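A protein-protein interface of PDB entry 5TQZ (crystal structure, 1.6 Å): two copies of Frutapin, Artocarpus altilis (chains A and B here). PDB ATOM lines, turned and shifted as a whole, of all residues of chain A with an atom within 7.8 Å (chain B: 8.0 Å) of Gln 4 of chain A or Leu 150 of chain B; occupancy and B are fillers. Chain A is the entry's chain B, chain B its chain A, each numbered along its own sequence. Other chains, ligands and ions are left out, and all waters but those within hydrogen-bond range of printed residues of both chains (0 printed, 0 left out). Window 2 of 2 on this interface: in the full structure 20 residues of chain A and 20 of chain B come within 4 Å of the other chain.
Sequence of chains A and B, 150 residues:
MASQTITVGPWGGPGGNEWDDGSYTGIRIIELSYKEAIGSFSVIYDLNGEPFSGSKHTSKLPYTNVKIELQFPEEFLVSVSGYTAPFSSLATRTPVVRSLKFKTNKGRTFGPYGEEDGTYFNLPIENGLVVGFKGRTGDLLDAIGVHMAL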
ATOM      1  N   MET A   1      27.376   7.672   9.850  1.00  0.00           N
ATOM      2  CA  MET A   1      27.067   7.142  11.245  1.00  0.00           C
ATOM      3  C   MET A   1      25.631   6.439  11.533  1.00  0.00           C
ATOM      4  O   MET A   1      25.368   5.352  11.005  1.00  0.00           O
ATOM      5  CB  MET A   1      27.556   8.131  12.363  1.00  0.00           C
ATOM      6  CG  MET A   1      27.207   9.664  12.299  1.00  0.00           C
ATOM      7  SD  MET A   1      26.115  10.118  10.946  1.00  0.00           S
ATOM      8  CE  MET A   1      25.628  11.863  11.235  1.00  0.00           C
ATOM      9  N   ALA A   2      24.851   7.008  12.438  1.00  0.00           N
ATOM     10  CA  ALA A   2      23.631   6.406  12.981  1.00  0.00           C
ATOM     11  C   ALA A   2      22.421   6.830  12.131  1.00  0.00           C
ATOM     12  O   ALA A   2      22.474   7.743  11.264  1.00  0.00           O
ATOM     13  CB  ALA A   2      23.483   6.904  14.433  1.00  0.00           C
ATOM     14  N   SER A   3      21.290   6.096  12.301  1.00  0.00           N
ATOM     15  CA  SER A   3      20.063   6.455  11.500  1.00  0.00           C
ATOM     16  C   SER A   3      19.684   7.926  11.864  1.00  0.00           C
ATOM     17  O   SER A   3      19.652   8.291  13.023  1.00  0.00           O
ATOM     18  CB  SER A   3      18.957   5.496  11.827  1.00  0.00           C
ATOM     19  OG  SER A   3      17.903   5.501  10.833  1.00  0.00           O
ATOM     20  N   GLN A   4      19.084   8.550  10.815  1.00  0.00           N
ATOM     21  CA  GLN A   4      18.588   9.956  10.863  1.00  0.00           C
ATOM     22  C   GLN A   4      17.200  10.125  10.353  1.00  0.00           C
ATOM     23  O   GLN A   4      16.659   9.294   9.670  1.00  0.00           O
ATOM     24  CB  GLN A   4      19.440  10.847   9.988  1.00  0.00           C
ATOM     25  CG  GLN A   4      19.550  10.449   8.531  1.00  0.00           C
ATOM     26  CD  GLN A   4      20.732  11.169   7.947  1.00  0.00           C
ATOM     27  OE1 GLN A   4      20.584  12.155   7.147  1.00  0.00           O
ATOM     28  NE2 GLN A   4      21.919  10.841   8.501  1.00  0.00           N
ATOM     29  N   THR A   5      16.654  11.338  10.679  1.00  0.00           N
ATOM     30  CA  THR A   5      15.289  11.682  10.283  1.00  0.00           C
ATOM     31  C   THR A   5      15.438  13.099   9.703  1.00  0.00           C
ATOM     32  O   THR A   5      16.232  13.884  10.129  1.00  0.00           O
ATOM     33  CB  THR A   5      14.313  11.716  11.477  1.00  0.00           C
ATOM     34  OG1 THR A   5      14.881  12.577  12.516  1.00  0.00           O
ATOM     35  CG2 THR A   5      14.006  10.321  12.143  1.00  0.00           C
ATOM     36  N   ILE A   6      14.498  13.417   8.847  1.00  0.00           N
ATOM     37  CA  ILE A   6      14.190  14.798   8.490  1.00  0.00           C
ATOM     38  C   ILE A   6      13.868  15.610   9.677  1.00  0.00           C
ATOM     39  O   ILE A   6      13.165  15.245  10.565  1.00  0.00           O
ATOM     40  CB  ILE A   6      13.067  14.762   7.426  1.00  0.00           C
ATOM     41  CG1 ILE A   6      13.614  14.239   6.096  1.00  0.00           C
ATOM     42  CG2 ILE A   6      12.503  16.112   7.169  1.00  0.00           C
ATOM     43  CD1 ILE A   6      12.549  14.173   4.982  1.00  0.00           C
ATOM     44  N   THR A   7      14.499  16.764   9.783  1.00  0.00           N
ATOM     45  CA  THR A   7      14.324  17.625  10.912  1.00  0.00           C
ATOM     46  C   THR A   7      14.136  19.044  10.386  1.00  0.00           C
ATOM     47  O   THR A   7      14.756  19.519   9.435  1.00  0.00           O
ATOM     48  CB  THR A   7      15.585  17.626  11.780  1.00  0.00           C
ATOM     49  OG1 THR A   7      15.879  16.288  12.086  1.00  0.00           O
ATOM     50  CG2 THR A   7      15.441  18.395  12.993  1.00  0.00           C
ATOM     51  N   SER A  23      14.820  10.661  17.954  1.00  0.00           N
ATOM     52  CA  SER A  23      13.677  10.154  17.200  1.00  0.00           C
ATOM     53  C   SER A  23      13.247   8.777  17.746  1.00  0.00           C
ATOM     54  O   SER A  23      14.062   7.965  18.251  1.00  0.00           O
ATOM     55  CB  SER A  23      13.934  10.038  15.718  1.00  0.00           C
ATOM     56  OG  SER A  23      15.069   9.246  15.392  1.00  0.00           O
ATOM     57  N   VAL A 131       8.130  12.330  15.017  1.00  0.00           N
ATOM     58  CA  VAL A 131       8.779  11.296  15.755  1.00  0.00           C
ATOM     59  C   VAL A 131       9.787  11.779  16.827  1.00  0.00           C
ATOM     60  O   VAL A 131      10.428  10.991  17.509  1.00  0.00           O
ATOM     61  CB  VAL A 131       9.398  10.262  14.865  1.00  0.00           C
ATOM     62  CG1 VAL A 131       8.352   9.565  13.945  1.00  0.00           C
ATOM     63  CG2 VAL A 131      10.490  10.919  14.108  1.00  0.00           C
ATOM     64  N   HIS A 147      11.575  16.448  14.493  1.00  0.00           N
ATOM     65  CA  HIS A 147      11.975  15.399  13.655  1.00  0.00           C
ATOM     66  C   HIS A 147      10.689  14.747  13.016  1.00  0.00           C
ATOM     67  O   HIS A 147       9.725  14.448  13.743  1.00  0.00           O
ATOM     68  CB  HIS A 147      12.714  14.409  14.472  1.00  0.00           C
ATOM     69  CG  HIS A 147      13.924  14.941  15.144  1.00  0.00           C
ATOM     70  ND1 HIS A 147      15.114  15.300  14.534  1.00  0.00           N
ATOM     71  CD2 HIS A 147      14.234  14.901  16.460  1.00  0.00           C
ATOM     72  CE1 HIS A 147      16.007  15.662  15.443  1.00  0.00           C
ATOM     73  NE2 HIS A 147      15.520  15.383  16.603  1.00  0.00           N
ATOM     74  N   MET A 148      10.892  14.322  11.768  1.00  0.00           N
ATOM     75  CA  MET A 148       9.744  13.729  10.996  1.00  0.00           C
ATOM     76  C   MET A 148      10.179  12.377  10.296  1.00  0.00           C
ATOM     77  O   MET A 148      11.359  12.146   9.852  1.00  0.00           O
ATOM     78  CB  MET A 148       9.061  14.678  10.017  1.00  0.00           C
ATOM     79  CG  MET A 148       8.618  15.994  10.648  1.00  0.00           C
ATOM     80  SD  MET A 148       7.765  16.944   9.397  1.00  0.00           S
ATOM     81  CE  MET A 148       6.291  16.020   9.174  1.00  0.00           C
ATOM     82  N   ALA A 149       9.228  11.464  10.311  1.00  0.00           N
ATOM     83  CA  ALA A 149       9.454  10.202   9.556  1.00  0.00           C
ATOM     84  C   ALA A 149       8.154   9.716   8.936  1.00  0.00           C
ATOM     85  O   ALA A 149       7.088  10.150   9.392  1.00  0.00           O
ATOM     86  CB  ALA A 149      10.023   9.168  10.501  1.00  0.00           C
ATOM     87  N   THR B   5       6.491  10.610   0.011  1.00  0.00           N
ATOM     88  CA  THR B   5       7.502  11.390   0.741  1.00  0.00           C
ATOM     89  C   THR B   5       6.808  12.153   1.815  1.00  0.00           C
ATOM     90  O   THR B   5       5.534  12.352   1.863  1.00  0.00           O
ATOM     91  CB  THR B   5       8.160  12.516  -0.151  1.00  0.00           C
ATOM     92  OG1 THR B   5       7.133  13.324  -0.771  1.00  0.00           O
ATOM     93  CG2 THR B   5       8.994  11.912  -1.271  1.00  0.00           C
ATOM     94  N   ILE B   6       7.601  12.561   2.793  1.00  0.00           N
ATOM     95  CA  ILE B   6       7.129  13.493   3.819  1.00  0.00           C
ATOM     96  C   ILE B   6       6.705  14.736   3.097  1.00  0.00           C
ATOM     97  O   ILE B   6       7.442  15.305   2.256  1.00  0.00           O
ATOM     98  CB  ILE B   6       8.227  13.808   4.819  1.00  0.00           C
ATOM     99  CG1 ILE B   6       8.462  12.571   5.738  1.00  0.00           C
ATOM    100  CG2 ILE B   6       7.915  15.143   5.548  1.00  0.00           C
ATOM    101  CD1 ILE B   6       9.372  12.645   6.856  1.00  0.00           C
ATOM    102  N   TYR B  24      11.275  13.879  -6.774  1.00  0.00           N
ATOM    103  CA  TYR B  24      12.458  13.748  -7.578  1.00  0.00           C
ATOM    104  C   TYR B  24      13.745  13.561  -6.758  1.00  0.00           C
ATOM    105  O   TYR B  24      13.679  13.235  -5.602  1.00  0.00           O
ATOM    106  CB  TYR B  24      12.576  14.946  -8.564  1.00  0.00           C
ATOM    107  CG  TYR B  24      11.398  15.188  -9.357  1.00  0.00           C
ATOM    108  CD1 TYR B  24      10.330  15.962  -8.856  1.00  0.00           C
ATOM    109  CD2 TYR B  24      11.277  14.643 -10.620  1.00  0.00           C
ATOM    110  CE1 TYR B  24       9.140  16.123  -9.613  1.00  0.00           C
ATOM    111  CE2 TYR B  24      10.179  14.944 -11.379  1.00  0.00           C
ATOM    112  CZ  TYR B  24       9.126  15.695 -10.892  1.00  0.00           C
ATOM    113  OH  TYR B  24       7.928  15.914 -11.589  1.00  0.00           O
ATOM    114  N   THR B  25      14.976  13.769  -7.302  1.00  0.00           N
ATOM    115  CA  THR B  25      16.173  13.632  -6.473  1.00  0.00           C
ATOM    116  C   THR B  25      16.703  14.918  -5.926  1.00  0.00           C
ATOM    117  O   THR B  25      17.581  14.956  -4.998  1.00  0.00           O
ATOM    118  CB  THR B  25      17.265  12.837  -7.221  1.00  0.00           C
ATOM    119  OG1 THR B  25      17.250  13.054  -8.576  1.00  0.00           O
ATOM    120  CG2 THR B  25      16.919  11.302  -7.078  1.00  0.00           C
ATOM    121  N   ASN B 127      17.717  19.138   8.596  1.00  0.00           N
ATOM    122  CA  ASN B 127      18.241  17.984   7.839  1.00  0.00           C
ATOM    123  C   ASN B 127      17.221  17.455   6.897  1.00  0.00           C
ATOM    124  O   ASN B 127      16.045  17.382   7.254  1.00  0.00           O
ATOM    125  CB  ASN B 127      18.501  16.910   8.825  1.00  0.00           C
ATOM    126  CG  ASN B 127      19.289  15.716   8.212  1.00  0.00           C
ATOM    127  OD1 ASN B 127      20.282  15.858   7.446  1.00  0.00           O
ATOM    128  ND2 ASN B 127      18.919  14.511   8.644  1.00  0.00           N
ATOM    129  N   GLY B 128      17.575  17.099   5.668  1.00  0.00           N
ATOM    130  CA  GLY B 128      16.667  16.682   4.591  1.00  0.00           C
ATOM    131  C   GLY B 128      16.777  17.600   3.389  1.00  0.00           C
ATOM    132  O   GLY B 128      17.558  18.629   3.469  1.00  0.00           O
ATOM    133  N   LEU B 129      16.029  17.194   2.329  1.00  0.00           N
ATOM    134  CA  LEU B 129      16.148  17.879   1.081  1.00  0.00           C
ATOM    135  C   LEU B 129      14.769  18.063   0.508  1.00  0.00           C
ATOM    136  O   LEU B 129      13.922  17.144   0.642  1.00  0.00           O
ATOM    137  CB  LEU B 129      17.040  17.070   0.085  1.00  0.00           C
ATOM    138  CG  LEU B 129      18.507  16.984   0.172  1.00  0.00           C
ATOM    139  CD1 LEU B 129      19.078  16.127  -0.996  1.00  0.00           C
ATOM    140  CD2 LEU B 129      19.164  18.344   0.201  1.00  0.00           C
ATOM    141  N   VAL B 130      14.547  19.219  -0.054  1.00  0.00           N
ATOM    142  CA  VAL B 130      13.379  19.481  -0.829  1.00  0.00           C
ATOM    143  C   VAL B 130      13.490  18.673  -2.138  1.00  0.00           C
ATOM    144  O   VAL B 130      14.517  18.774  -2.877  1.00  0.00           O
ATOM    145  CB  VAL B 130      13.209  20.961  -1.214  1.00  0.00           C
ATOM    146  CG1 VAL B 130      11.991  21.110  -2.136  1.00  0.00           C
ATOM    147  CG2 VAL B 130      13.040  21.793   0.083  1.00  0.00           C
ATOM    148  N   VAL B 131      12.511  17.800  -2.359  1.00  0.00           N
ATOM    149  CA  VAL B 131      12.440  16.979  -3.475  1.00  0.00           C
ATOM    150  C   VAL B 131      11.349  17.227  -4.516  1.00  0.00           C
ATOM    151  O   VAL B 131      11.241  16.435  -5.456  1.00  0.00           O
ATOM    152  CB  VAL B 131      12.601  15.462  -3.185  1.00  0.00           C
ATOM    153  CG1 VAL B 131      13.930  15.127  -2.551  1.00  0.00           C
ATOM    154  CG2 VAL B 131      11.547  14.920  -2.327  1.00  0.00           C
ATOM    155  N   MET B 148       9.693  16.288   0.806  1.00  0.00           N
ATOM    156  CA  MET B 148      11.055  16.259   1.471  1.00  0.00           C
ATOM    157  C   MET B 148      11.514  14.756   1.589  1.00  0.00           C
ATOM    158  O   MET B 148      10.678  13.873   1.786  1.00  0.00           O
ATOM    159  CB  MET B 148      11.024  16.900   2.881  1.00  0.00           C
ATOM    160  CG  MET B 148      10.490  18.297   2.898  1.00  0.00           C
ATOM    161  SD  MET B 148      10.548  18.938   4.618  1.00  0.00           S
ATOM    162  CE  MET B 148      12.312  18.977   4.729  1.00  0.00           C
ATOM    163  N   ALA B 149      12.796  14.535   1.446  1.00  0.00           N
ATOM    164  CA  ALA B 149      13.357  13.197   1.546  1.00  0.00           C
ATOM    165  C   ALA B 149      14.726  13.378   2.052  1.00  0.00           C
ATOM    166  O   ALA B 149      15.192  14.513   2.049  1.00  0.00           O
ATOM    167  CB  ALA B 149      13.443  12.548   0.216  1.00  0.00           C
ATOM    168  N   LEU B 150      15.269  12.286   2.535  1.00  0.00           N
ATOM    169  CA  LEU B 150      16.494  12.133   3.427  1.00  0.00           C
ATOM    170  C   LEU B 150      16.430  11.827   5.027  1.00  0.00           C
ATOM    171  O   LEU B 150      15.934  10.777   5.490  1.00  0.00           O
ATOM    172  CB  LEU B 150      17.569  13.106   3.026  1.00  0.00           C
ATOM    173  CG  LEU B 150      18.481  12.329   1.983  1.00  0.00           C
ATOM    174  CD1 LEU B 150      17.572  11.973   0.848  1.00  0.00           C
ATOM    175  CD2 LEU B 150      19.741  13.103   1.536  1.00  0.00           C
ATOM    176  OXT LEU B 150      16.948  12.549   6.014  1.00  0.00           O
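Of the 12 printed residues of chain A, 6 touch a printed residue of chain B. Printed residues of chain A that touch a printed residue of chain B: Gln 4, Thr 5, Ile 6, Thr 7, Met 148 and Ala 149. Hydrophobic or aromatic side chains of chain A within 4 Å of the printed part of chain B: Ile 6 and Met 148. Hydrophobic or aromatic side chains of chain B within 4 Å of the printed part of chain A: Ile 6 and Met 148. Among the printed residues, 11 pairs touch across the chains. Among the printed residues, no Asp or Glu carboxylate lies within 4 Å of a Lys or Arg side-chain nitrogen of the other chain.
Among the printed residues, merely in contact across the chains: Gln 4 of chain A with Leu 150 of chain B (3.8 Å), Ile 6 of chain A with Ile 6 of chain B (3.99 Å), Ile 6 of chain A with Asn 127 of chain B (3.4 Å), Ile 6 of chain A with Met 148 of chain B (3.6 Å), Ile 6 of chain A with Ala 149 of chain B (3.6 Å), Ile 6 of chain A with Leu 150 of chain B (3.7 Å), Met 148 of chain A with Ile 6 of chain B (3.5 Å) and Ala 149 of chain A with Ile 6 of chain B (3.6 Å).
The backbone NH (N) of Met 148 of chain B is in hydrogen-bond range of the backbone carbonyl oxygen (O) of Ile 6 of chain B, 2.9 Å away. N of Leu 129 of chain B lies within hydrogen-bond range of O of Ala 149 of chain B, 2.8 Å away. The backbone carbonyl oxygen of Thr 5 of chain A sits at hydrogen-bond distance from the side-chain hydroxyl of Thr 7 of chain A, at 3.1 Å. The side-chain hydroxyl of Thr 5 of chain A sits at hydrogen-bond distance from a ring nitrogen (ND1) of His 147 of chain A (3.4 Å). O of Ile 6 of chain A lies within hydrogen-bond range of N of Met 148 of chain A (2.7 Å). OG1 of Thr 7 of chain A is in hydrogen-bond range of ND1 of His 147 of chain A, 2.7 Å away.
Ile 6 of chain A touches its own counterpart, Ile 6 of chain B. Ile 6 of chain A touches Met 148 of chain B, and with the chains exchanged Met 148 of chain A touches Ile 6 of chain B. Ile 6 of chain A touches Ala 149 of chain B, and with the chains exchanged Ala 149 of chain A touches Ile 6 of chain B. Positions printed for both chains: 5, 6, 131, 148 and 149.
ND2 of Asn 127 of chain B lies within hydrogen-bond range of OE1 of Gln 4 of chain A, 3.3 Å away. The backbone carbonyl oxygen (O) of Thr 5 of chain A sits at hydrogen-bond distance from the side-chain amide nitrogen (ND2) of Asn 127 of chain B, 3.1 Å away. The backbone carbonyl oxygen (O) of Asn 127 of chain B sits at hydrogen-bond distance from the backbone NH (N) of Thr 7 of chain A, 3.0 Å away.
Of chain B, only Asn 127 (3.3 Å) and Leu 150 (3.8 Å) come within 4 Å of Gln 4 of chain A. Of chain A, only Gln 4 and Ile 6 come within 4 Å of Leu 150 of chain B. Ala 149 of chain B touches just one residue of chain A: Ile 6. Of the printed residues of chain B, Met 148 of chain A touches Ile 6. Of the printed residues of chain B, Thr 7 of chain A touches Asn 127. Of the printed residues of chain A, Ile 6 of chain B touches Ile 6 (3.99 Å), Met 148 (3.5 Å) and Ala 149 (3.6 Å). Of the printed residues of chain B, Ile 6 of chain A touches Ile 6, Asn 127, Met 148, Ala 149 and Leu 150. The nearest residue of chain B that does not touch Gln 4 of chain A is Gly 128 of chain B (6.0 Å).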
